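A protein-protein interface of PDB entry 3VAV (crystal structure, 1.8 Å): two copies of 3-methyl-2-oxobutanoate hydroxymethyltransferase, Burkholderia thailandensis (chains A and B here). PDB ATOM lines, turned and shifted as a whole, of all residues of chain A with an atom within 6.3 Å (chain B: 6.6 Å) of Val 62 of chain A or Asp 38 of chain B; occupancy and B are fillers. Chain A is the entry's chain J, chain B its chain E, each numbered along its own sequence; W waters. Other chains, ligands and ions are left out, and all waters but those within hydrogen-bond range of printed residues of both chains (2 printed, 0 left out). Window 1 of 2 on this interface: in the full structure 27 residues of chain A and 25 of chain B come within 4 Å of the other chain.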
ATOM      1  N   THR A  35      32.981  30.199 -29.426  1.00  0.00           N
ATOM      2  CA  THR A  35      31.981  30.090 -28.354  1.00  0.00           C
ATOM      3  C   THR A  35      31.602  28.636 -28.175  1.00  0.00           C
ATOM      4  O   THR A  35      31.789  27.789 -29.071  1.00  0.00           O
ATOM      5  CB  THR A  35      30.734  30.966 -28.556  1.00  0.00           C
ATOM      6  OG1 THR A  35      29.975  30.522 -29.680  1.00  0.00           O
ATOM      7  CG2 THR A  35      31.094  32.447 -28.659  1.00  0.00           C
ATOM      8  N   TYR A  37      28.824  26.198 -25.409  1.00  0.00           N
ATOM      9  CA  TYR A  37      27.811  26.339 -24.336  1.00  0.00           C
ATOM     10  C   TYR A  37      27.341  25.024 -23.745  1.00  0.00           C
ATOM     11  O   TYR A  37      26.415  25.023 -22.956  1.00  0.00           O
ATOM     12  CB  TYR A  37      26.566  27.101 -24.849  1.00  0.00           C
ATOM     13  CG  TYR A  37      26.840  28.240 -25.825  1.00  0.00           C
ATOM     14  CD1 TYR A  37      27.155  29.515 -25.372  1.00  0.00           C
ATOM     15  CD2 TYR A  37      26.785  28.024 -27.216  1.00  0.00           C
ATOM     16  CE1 TYR A  37      27.387  30.571 -26.267  1.00  0.00           C
ATOM     17  CE2 TYR A  37      27.027  29.060 -28.121  1.00  0.00           C
ATOM     18  CZ  TYR A  37      27.324  30.340 -27.651  1.00  0.00           C
ATOM     19  OH  TYR A  37      27.582  31.382 -28.542  1.00  0.00           O
ATOM     20  N   SER A  58      26.171  35.711 -26.456  1.00  0.00           N
ATOM     21  CA  SER A  58      25.623  35.331 -27.755  1.00  0.00           C
ATOM     22  C   SER A  58      24.606  34.175 -27.653  1.00  0.00           C
ATOM     23  O   SER A  58      23.754  34.024 -28.502  1.00  0.00           O
ATOM     24  CB  SER A  58      26.762  34.932 -28.699  1.00  0.00           C
ATOM     25  OG  SER A  58      27.689  34.043 -28.075  1.00  0.00           O
ATOM     26  N   LEU A  59      24.702  33.394 -26.593  1.00  0.00           N
ATOM     27  CA  LEU A  59      23.707  32.343 -26.313  1.00  0.00           C
ATOM     28  C   LEU A  59      22.275  32.883 -26.236  1.00  0.00           C
ATOM     29  O   LEU A  59      21.331  32.163 -26.536  1.00  0.00           O
ATOM     30  CB  LEU A  59      24.093  31.546 -25.068  1.00  0.00           C
ATOM     31  CG  LEU A  59      23.950  32.146 -23.673  1.00  0.00           C
ATOM     32  CD1 LEU A  59      22.520  32.064 -23.127  1.00  0.00           C
ATOM     33  CD2 LEU A  59      24.945  31.490 -22.708  1.00  0.00           C
ATOM     34  N   GLY A  60      22.120  34.169 -25.870  1.00  0.00           N
ATOM     35  CA  GLY A  60      20.830  34.819 -25.915  1.00  0.00           C
ATOM     36  C   GLY A  60      20.188  34.746 -27.289  1.00  0.00           C
ATOM     37  O   GLY A  60      18.976  34.569 -27.391  1.00  0.00           O
ATOM     38  N   ASN A  61      21.001  34.907 -28.332  1.00  0.00           N
ATOM     39  CA  ASN A  61      20.535  34.797 -29.712  1.00  0.00           C
ATOM     40  C   ASN A  61      20.467  33.322 -30.127  1.00  0.00           C
ATOM     41  O   ASN A  61      19.390  32.796 -30.459  1.00  0.00           O
ATOM     42  CB  ASN A  61      21.491  35.513 -30.687  1.00  0.00           C
ATOM     43  CG  ASN A  61      21.537  36.998 -30.509  1.00  0.00           C
ATOM     44  OD1 ASN A  61      22.632  37.582 -30.414  1.00  0.00           O
ATOM     45  ND2 ASN A  61      20.380  37.646 -30.488  1.00  0.00           N
ATOM     46  N   VAL A  62      21.598  32.649 -30.055  1.00  0.00           N
ATOM     47  CA  VAL A  62      21.740  31.343 -30.705  1.00  0.00           C
ATOM     48  C   VAL A  62      21.063  30.209 -29.953  1.00  0.00           C
ATOM     49  O   VAL A  62      20.578  29.263 -30.580  1.00  0.00           O
ATOM     50  CB  VAL A  62      23.203  30.992 -31.072  1.00  0.00           C
ATOM     51  CG1 VAL A  62      23.765  31.998 -32.087  1.00  0.00           C
ATOM     52  CG2 VAL A  62      24.095  30.917 -29.843  1.00  0.00           C
ATOM     53  N   LEU A  63      21.042  30.251 -28.621  1.00  0.00           N
ATOM     54  CA  LEU A  63      20.329  29.221 -27.848  1.00  0.00           C
ATOM     55  C   LEU A  63      18.927  29.622 -27.431  1.00  0.00           C
ATOM     56  O   LEU A  63      17.971  28.832 -27.572  1.00  0.00           O
ATOM     57  CB  LEU A  63      21.122  28.826 -26.614  1.00  0.00           C
ATOM     58  CG  LEU A  63      22.565  28.378 -26.848  1.00  0.00           C
ATOM     59  CD1 LEU A  63      23.054  27.789 -25.527  1.00  0.00           C
ATOM     60  CD2 LEU A  63      22.708  27.350 -27.961  1.00  0.00           C
ATOM     61  N   GLN A  64      18.764  30.863 -26.958  1.00  0.00           N
ATOM     62  CA  GLN A  64      17.493  31.284 -26.348  1.00  0.00           C
ATOM     63  C   GLN A  64      16.507  31.864 -27.391  1.00  0.00           C
ATOM     64  O   GLN A  64      15.327  31.922 -27.151  1.00  0.00           O
ATOM     65  CB  GLN A  64      17.744  32.295 -25.223  1.00  0.00           C
ATOM     66  CG  GLN A  64      18.691  31.767 -24.150  1.00  0.00           C
ATOM     67  CD  GLN A  64      18.909  32.764 -23.031  1.00  0.00           C
ATOM     68  OE1 GLN A  64      18.628  33.933 -23.196  1.00  0.00           O
ATOM     69  NE2 GLN A  64      19.412  32.292 -21.885  1.00  0.00           N
ATOM     70  N   GLY A  65      17.021  32.248 -28.544  1.00  0.00           N
ATOM     71  CA  GLY A  65      16.194  32.753 -29.619  1.00  0.00           C
ATOM     72  C   GLY A  65      15.656  34.143 -29.373  1.00  0.00           C
ATOM     73  O   GLY A  65      14.604  34.536 -29.927  1.00  0.00           O
ATOM     74  N   GLN A  66      16.367  34.906 -28.543  1.00  0.00           N
ATOM     75  CA  GLN A  66      16.026  36.314 -28.304  1.00  0.00           C
ATOM     76  C   GLN A  66      16.668  37.169 -29.409  1.00  0.00           C
ATOM     77  O   GLN A  66      17.647  36.754 -30.051  1.00  0.00           O
ATOM     78  CB  GLN A  66      16.557  36.751 -26.931  1.00  0.00           C
ATOM     79  CG  GLN A  66      16.061  35.923 -25.749  1.00  0.00           C
ATOM     80  CD  GLN A  66      14.760  36.464 -25.129  1.00  0.00           C
ATOM     81  OE1 GLN A  66      14.013  37.207 -25.771  1.00  0.00           O
ATOM     82  NE2 GLN A  66      14.496  36.094 -23.890  1.00  0.00           N
ATOM     83  N   VAL A 226      31.142  32.875 -33.218  1.00  0.00           N
ATOM     84  CA  VAL A 226      30.064  32.137 -32.562  1.00  0.00           C
ATOM     85  C   VAL A 226      29.988  30.759 -33.212  1.00  0.00           C
ATOM     86  O   VAL A 226      29.955  30.662 -34.439  1.00  0.00           O
ATOM     87  CB  VAL A 226      28.711  32.876 -32.713  1.00  0.00           C
ATOM     88  CG1 VAL A 226      27.533  31.988 -32.258  1.00  0.00           C
ATOM     89  CG2 VAL A 226      28.752  34.222 -31.984  1.00  0.00           C
ATOM     90  N   HIS A 228      27.670  28.531 -33.719  1.00  0.00           N
ATOM     91  CA  HIS A 228      26.585  28.203 -34.645  1.00  0.00           C
ATOM     92  C   HIS A 228      26.785  28.875 -35.980  1.00  0.00           C
ATOM     93  O   HIS A 228      26.389  28.339 -37.034  1.00  0.00           O
ATOM     94  CB  HIS A 228      25.240  28.566 -34.021  1.00  0.00           C
ATOM     95  CG  HIS A 228      24.961  27.806 -32.774  1.00  0.00           C
ATOM     96  ND1 HIS A 228      25.679  27.983 -31.638  1.00  0.00           N
ATOM     97  CD2 HIS A 228      24.067  26.782 -32.515  1.00  0.00           C
ATOM     98  CE1 HIS A 228      25.247  27.129 -30.697  1.00  0.00           C
ATOM     99  NE2 HIS A 228      24.268  26.380 -31.230  1.00  0.00           N
ATOM    100  N   ASP A 229      27.411  30.044 -35.967  1.00  0.00           N
ATOM    101  CA  ASP A 229      27.775  30.715 -37.238  1.00  0.00           C
ATOM    102  C   ASP A 229      28.753  29.879 -38.057  1.00  0.00           C
ATOM    103  O   ASP A 229      28.580  29.674 -39.287  1.00  0.00           O
ATOM    104  CB  ASP A 229      28.359  32.115 -36.971  1.00  0.00           C
ATOM    105  CG  ASP A 229      27.297  33.147 -36.651  1.00  0.00           C
ATOM    106  OD1 ASP A 229      26.090  32.963 -37.015  1.00  0.00           O
ATOM    107  OD2 ASP A 229      27.653  34.148 -35.997  1.00  0.00           O
ATOM    108  N   PHE A 234      22.453  28.706 -39.769  1.00  0.00           N
ATOM    109  CA  PHE A 234      21.453  29.738 -40.072  1.00  0.00           C
ATOM    110  C   PHE A 234      21.233  29.846 -41.587  1.00  0.00           C
ATOM    111  O   PHE A 234      22.183  29.688 -42.358  1.00  0.00           O
ATOM    112  CB  PHE A 234      21.907  31.083 -39.490  1.00  0.00           C
ATOM    113  CG  PHE A 234      22.003  31.060 -38.012  1.00  0.00           C
ATOM    114  CD1 PHE A 234      20.850  30.914 -37.250  1.00  0.00           C
ATOM    115  CD2 PHE A 234      23.246  31.051 -37.370  1.00  0.00           C
ATOM    116  CE1 PHE A 234      20.923  30.843 -35.857  1.00  0.00           C
ATOM    117  CE2 PHE A 234      23.332  30.974 -35.999  1.00  0.00           C
ATOM    118  CZ  PHE A 234      22.164  30.868 -35.233  1.00  0.00           C
ATOM    119  N   CYS B  36      15.725  18.081 -29.110  1.00  0.00           N
ATOM    120  CA  CYS B  36      16.122  19.434 -29.468  1.00  0.00           C
ATOM    121  C   CYS B  36      16.071  20.260 -28.192  1.00  0.00           C
ATOM    122  O   CYS B  36      15.187  20.044 -27.346  1.00  0.00           O
ATOM    123  CB  CYS B  36      15.169  20.003 -30.519  1.00  0.00           C
ATOM    124  SG  CYS B  36      15.764  21.560 -31.179  1.00  0.00           S
ATOM    125  N   TYR B  37      17.035  21.158 -28.018  1.00  0.00           N
ATOM    126  CA  TYR B  37      17.217  21.840 -26.743  1.00  0.00           C
ATOM    127  C   TYR B  37      17.468  23.336 -26.845  1.00  0.00           C
ATOM    128  O   TYR B  37      17.761  23.981 -25.831  1.00  0.00           O
ATOM    129  CB  TYR B  37      18.366  21.208 -25.940  1.00  0.00           C
ATOM    130  CG  TYR B  37      18.487  19.696 -26.024  1.00  0.00           C
ATOM    131  CD1 TYR B  37      17.714  18.865 -25.222  1.00  0.00           C
ATOM    132  CD2 TYR B  37      19.397  19.109 -26.897  1.00  0.00           C
ATOM    133  CE1 TYR B  37      17.835  17.457 -25.290  1.00  0.00           C
ATOM    134  CE2 TYR B  37      19.524  17.724 -26.987  1.00  0.00           C
ATOM    135  CZ  TYR B  37      18.754  16.896 -26.176  1.00  0.00           C
ATOM    136  OH  TYR B  37      18.918  15.515 -26.262  1.00  0.00           O
ATOM    137  N   ASP B  38      17.444  23.891 -28.062  1.00  0.00           N
ATOM    138  CA  ASP B  38      17.705  25.311 -28.250  1.00  0.00           C
ATOM    139  C   ASP B  38      17.025  25.857 -29.516  1.00  0.00           C
ATOM    140  O   ASP B  38      16.536  25.089 -30.343  1.00  0.00           O
ATOM    141  CB  ASP B  38      19.217  25.564 -28.289  1.00  0.00           C
ATOM    142  CG  ASP B  38      19.874  24.957 -29.482  1.00  0.00           C
ATOM    143  OD1 ASP B  38      19.596  25.433 -30.614  1.00  0.00           O
ATOM    144  OD2 ASP B  38      20.657  23.964 -29.304  1.00  0.00           O
ATOM    145  N   ALA B  39      17.001  27.190 -29.651  1.00  0.00           N
ATOM    146  CA  ALA B  39      16.220  27.859 -30.702  1.00  0.00           C
ATOM    147  C   ALA B  39      16.812  27.688 -32.105  1.00  0.00           C
ATOM    148  O   ALA B  39      16.071  27.655 -33.091  1.00  0.00           O
ATOM    149  CB  ALA B  39      16.070  29.339 -30.385  1.00  0.00           C
ATOM    150  N   SER B  40      18.143  27.619 -32.198  1.00  0.00           N
ATOM    151  CA  SER B  40      18.827  27.510 -33.507  1.00  0.00           C
ATOM    152  C   SER B  40      18.549  26.151 -34.141  1.00  0.00           C
ATOM    153  O   SER B  40      18.166  26.060 -35.311  1.00  0.00           O
ATOM    154  CB  SER B  40      20.328  27.730 -33.345  1.00  0.00           C
ATOM    155  OG  SER B  40      20.593  29.110 -33.112  1.00  0.00           O
ATOM    156  N   PHE B  41      18.660  25.097 -33.350  1.00  0.00           N
ATOM    157  CA  PHE B  41      18.304  23.779 -33.862  1.00  0.00           C
ATOM    158  C   PHE B  41      16.799  23.599 -34.004  1.00  0.00           C
ATOM    159  O   PHE B  41      16.362  22.929 -34.933  1.00  0.00           O
ATOM    160  CB  PHE B  41      18.950  22.658 -33.041  1.00  0.00           C
ATOM    161  CG  PHE B  41      20.416  22.429 -33.380  1.00  0.00           C
ATOM    162  CD1 PHE B  41      20.773  21.696 -34.483  1.00  0.00           C
ATOM    163  CD2 PHE B  41      21.419  23.000 -32.613  1.00  0.00           C
ATOM    164  CE1 PHE B  41      22.104  21.516 -34.823  1.00  0.00           C
ATOM    165  CE2 PHE B  41      22.752  22.826 -32.945  1.00  0.00           C
ATOM    166  CZ  PHE B  41      23.087  22.057 -34.051  1.00  0.00           C
ATOM    167  N   ALA B  42      15.991  24.199 -33.129  1.00  0.00           N
ATOM    168  CA  ALA B  42      14.526  24.169 -33.344  1.00  0.00           C
ATOM    169  C   ALA B  42      14.169  24.649 -34.759  1.00  0.00           C
ATOM    170  O   ALA B  42      13.409  23.997 -35.468  1.00  0.00           O
ATOM    171  CB  ALA B  42      13.768  24.980 -32.292  1.00  0.00           C
ATOM    172  N   ALA B  43      14.760  25.766 -35.177  1.00  0.00           N
ATOM    173  CA  ALA B  43      14.484  26.335 -36.484  1.00  0.00           C
ATOM    174  C   ALA B  43      14.999  25.437 -37.586  1.00  0.00           C
ATOM    175  O   ALA B  43      14.306  25.214 -38.588  1.00  0.00           O
ATOM    176  CB  ALA B  43      15.103  27.726 -36.593  1.00  0.00           C
ATOM    177  N   GLN B  53       9.628  17.653 -31.803  1.00  0.00           N
ATOM    178  CA  GLN B  53      10.867  17.998 -31.147  1.00  0.00           C
ATOM    179  C   GLN B  53      10.741  17.683 -29.658  1.00  0.00           C
ATOM    180  O   GLN B  53       9.778  18.111 -29.027  1.00  0.00           O
ATOM    181  CB  GLN B  53      11.198  19.476 -31.369  1.00  0.00           C
ATOM    182  CG  GLN B  53      11.403  19.830 -32.834  1.00  0.00           C
ATOM    183  CD  GLN B  53      11.949  21.258 -33.066  1.00  0.00           C
ATOM    184  OE1 GLN B  53      12.436  21.921 -32.128  1.00  0.00           O
ATOM    185  NE2 GLN B  53      11.888  21.735 -34.339  1.00  0.00           N
ATOM    186  N   ILE B  55      12.267  17.920 -25.882  1.00  0.00           N
ATOM    187  CA  ILE B  55      13.203  18.419 -24.854  1.00  0.00           C
ATOM    188  C   ILE B  55      13.360  17.292 -23.817  1.00  0.00           C
ATOM    189  O   ILE B  55      12.594  17.188 -22.846  1.00  0.00           O
ATOM    190  CB  ILE B  55      12.779  19.738 -24.190  1.00  0.00           C
ATOM    191  CG1 ILE B  55      12.751  20.903 -25.181  1.00  0.00           C
ATOM    192  CG2 ILE B  55      13.778  20.131 -23.091  1.00  0.00           C
ATOM    193  CD1 ILE B  55      11.428  21.126 -25.850  1.00  0.00           C
ATOM    194  N   LEU B  63      24.264  17.760 -23.044  1.00  0.00           N
ATOM    195  CA  LEU B  63      24.563  19.153 -22.726  1.00  0.00           C
ATOM    196  C   LEU B  63      25.320  19.329 -21.418  1.00  0.00           C
ATOM    197  O   LEU B  63      26.265  20.102 -21.362  1.00  0.00           O
ATOM    198  CB  LEU B  63      23.293  20.016 -22.708  1.00  0.00           C
ATOM    199  CG  LEU B  63      22.413  19.965 -23.946  1.00  0.00           C
ATOM    200  CD1 LEU B  63      21.283  21.001 -23.826  1.00  0.00           C
ATOM    201  CD2 LEU B  63      23.252  20.183 -25.222  1.00  0.00           C
ATOM    202  N   HIS B  80      15.267  24.776 -21.325  1.00  0.00           N
ATOM    203  CA  HIS B  80      15.441  24.362 -22.700  1.00  0.00           C
ATOM    204  C   HIS B  80      14.134  24.331 -23.485  1.00  0.00           C
ATOM    205  O   HIS B  80      14.099  24.664 -24.659  1.00  0.00           O
ATOM    206  CB  HIS B  80      16.162  23.012 -22.719  1.00  0.00           C
ATOM    207  CG  HIS B  80      17.578  23.097 -22.218  1.00  0.00           C
ATOM    208  ND1 HIS B  80      18.598  23.558 -22.999  1.00  0.00           N
ATOM    209  CD2 HIS B  80      18.136  22.785 -20.998  1.00  0.00           C
ATOM    210  CE1 HIS B  80      19.734  23.550 -22.294  1.00  0.00           C
ATOM    211  NE2 HIS B  80      19.471  23.084 -21.075  1.00  0.00           N
ATOM    212  N   CYS B  83      13.517  27.867 -24.633  1.00  0.00           N
ATOM    213  CA  CYS B  83      14.430  28.150 -25.741  1.00  0.00           C
ATOM    214  C   CYS B  83      13.870  27.616 -27.044  1.00  0.00           C
ATOM    215  O   CYS B  83      13.823  28.327 -28.057  1.00  0.00           O
ATOM    216  CB  CYS B  83      15.803  27.515 -25.464  1.00  0.00           C
ATOM    217  SG  CYS B  83      16.751  28.299 -24.130  1.00  0.00           S
ATOM    218  N   VAL B  84      13.461  26.338 -27.038  1.00  0.00           N
ATOM    219  CA  VAL B  84      12.872  25.730 -28.236  1.00  0.00           C
ATOM    220  C   VAL B  84      11.580  26.446 -28.618  1.00  0.00           C
ATOM    221  O   VAL B  84      11.358  26.790 -29.801  1.00  0.00           O
ATOM    222  CB  VAL B  84      12.582  24.235 -28.024  1.00  0.00           C
ATOM    223  CG1 VAL B  84      11.741  23.697 -29.200  1.00  0.00           C
ATOM    224  CG2 VAL B  84      13.883  23.453 -27.897  1.00  0.00           C
ATOM    225  N   ALA B  87      11.511  29.797 -30.666  1.00  0.00           N
ATOM    226  CA  ALA B  87      11.643  29.648 -32.125  1.00  0.00           C
ATOM    227  C   ALA B  87      10.307  29.494 -32.851  1.00  0.00           C
ATOM    228  O   ALA B  87      10.276  29.553 -34.090  1.00  0.00           O
ATOM    229  CB  ALA B  87      12.532  28.452 -32.462  1.00  0.00           C
ATOM    230  N   LEU B 227      19.581  14.128 -30.839  1.00  0.00           N
ATOM    231  CA  LEU B 227      20.140  15.010 -31.857  1.00  0.00           C
ATOM    232  C   LEU B 227      21.628  14.797 -32.022  1.00  0.00           C
ATOM    233  O   LEU B 227      22.105  14.507 -33.124  1.00  0.00           O
ATOM    234  CB  LEU B 227      19.849  16.486 -31.515  1.00  0.00           C
ATOM    235  CG  LEU B 227      20.386  17.552 -32.454  1.00  0.00           C
ATOM    236  CD1 LEU B 227      19.760  17.404 -33.828  1.00  0.00           C
ATOM    237  CD2 LEU B 227      20.140  18.962 -31.873  1.00  0.00           C
ATOM    238  N   HIS B 228      22.375  14.957 -30.929  1.00  0.00           N
ATOM    239  CA  HIS B 228      23.843  14.908 -30.980  1.00  0.00           C
ATOM    240  C   HIS B 228      24.351  13.562 -31.472  1.00  0.00           C
ATOM    241  O   HIS B 228      25.379  13.493 -32.151  1.00  0.00           O
ATOM    242  CB  HIS B 228      24.431  15.258 -29.605  1.00  0.00           C
ATOM    243  CG  HIS B 228      24.063  16.640 -29.153  1.00  0.00           C
ATOM    244  ND1 HIS B 228      22.787  16.981 -28.844  1.00  0.00           N
ATOM    245  CD2 HIS B 228      24.814  17.799 -29.036  1.00  0.00           C
ATOM    246  CE1 HIS B 228      22.735  18.274 -28.527  1.00  0.00           C
ATOM    247  NE2 HIS B 228      23.971  18.789 -28.657  1.00  0.00           N
HETATM  248  O   HOH W   1      23.329  24.164 -29.688  1.00  0.00           O
HETATM  249  O   HOH W   2      18.336  31.265 -32.948  1.00  0.00           O
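The backbone carbonyl oxygen of Asp 38 of chain B is in hydrogen-bond range of the side-chain sulfur of Cys 36 of chain B.
The side-chain carboxylate (OD1) of Asp 38 of chain B sits at hydrogen-bond distance from the backbone NH (N) of Ser 40 of chain B (3.1 Å).
The side-chain carboxylate (OD1) of Asp 38 of chain B lies within hydrogen-bond range of the backbone NH (N) of Phe 41 of chain B, 2.9 Å away.
O of Leu 59 of chain A lies within hydrogen-bond range of N of Gln 64 of chain A (2.9 Å).
The backbone NH of Gly 65 of chain A sits at hydrogen-bond distance from the backbone carbonyl oxygen of Gly 60 of chain A (3.2 Å).
3 positions are printed for both chains.
Of the 10 pairs that touch across the chains among the printed residues, none has its exchanged pair printed and touching as well.
Among the printed residues, merely in contact across the chains: Phe 234 of chain A with Ser 40 of chain B, Gly 65 of chain A with Ala 39 of chain B, Leu 63 of chain A with Asp 38 of chain B, Gln 64 of chain A with Cys 83 of chain B, Gln 64 of chain A with Ala 39 of chain B, His 228 of chain A with Ser 40 of chain B and Val 62 of chain A with Asp 38 of chain B.
Water W1 bridges OD2 of Asp 38 of chain B and NE2 of His 228 of chain A.
Water W2 bridges the backbone carbonyl oxygen of Asn 61 of chain A (3.1 Å) and the side-chain hydroxyl of Ser 40 of chain B (3.1 Å).
The backbone NH (N) of Ala 39 of chain B sits at hydrogen-bond distance from the backbone carbonyl oxygen (O) of Leu 63 of chain A (2.8 Å).
OG of Ser 40 of chain B sits at hydrogen-bond distance from O of Val 62 of chain A (2.5 Å).
SG of Cys 83 of chain B lies close to O of Leu 63 of chain A (3.7 Å).
Of the printed residues of chain B, Val 62 of chain A touches Asp 38 (3.95 Å) and Ser 40 (2.5 Å).
Of the printed residues of chain B, Gln 64 of chain A touches Ala 39 (3.9 Å) and Cys 83 (3.8 Å).
Asp 38 of chain B touches just these residues of chain A: Val 62 (3.95 Å) and Leu 63 (3.6 Å).
Of the printed residues of chain A, Ala 39 of chain B touches Leu 63 (2.8 Å), Gln 64 (3.9 Å) and Gly 65 (3.5 Å).
Of the printed residues of chain A, Ser 40 of chain B touches Val 62 (2.5 Å), His 228 (3.9 Å) and Phe 234 (3.2 Å).
Of the 15 printed residues of chain A, 6 touch a printed residue of chain B.
Hydrophobic or aromatic side chains of chain A within 4 Å of the printed part of chain B: Val 62, Leu 63, His 228 and Phe 234.
Along chain A the printed residues that touch a printed residue of chain B span positions 62 to 234.
Hydrophobic or aromatic side chains of chain B within 4 Å of the printed part of chain A: Ala 39.
Among the printed residues, no Asp or Glu carboxylate lies within 4 Å of a Lys or Arg side-chain nitrogen of the other chain.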
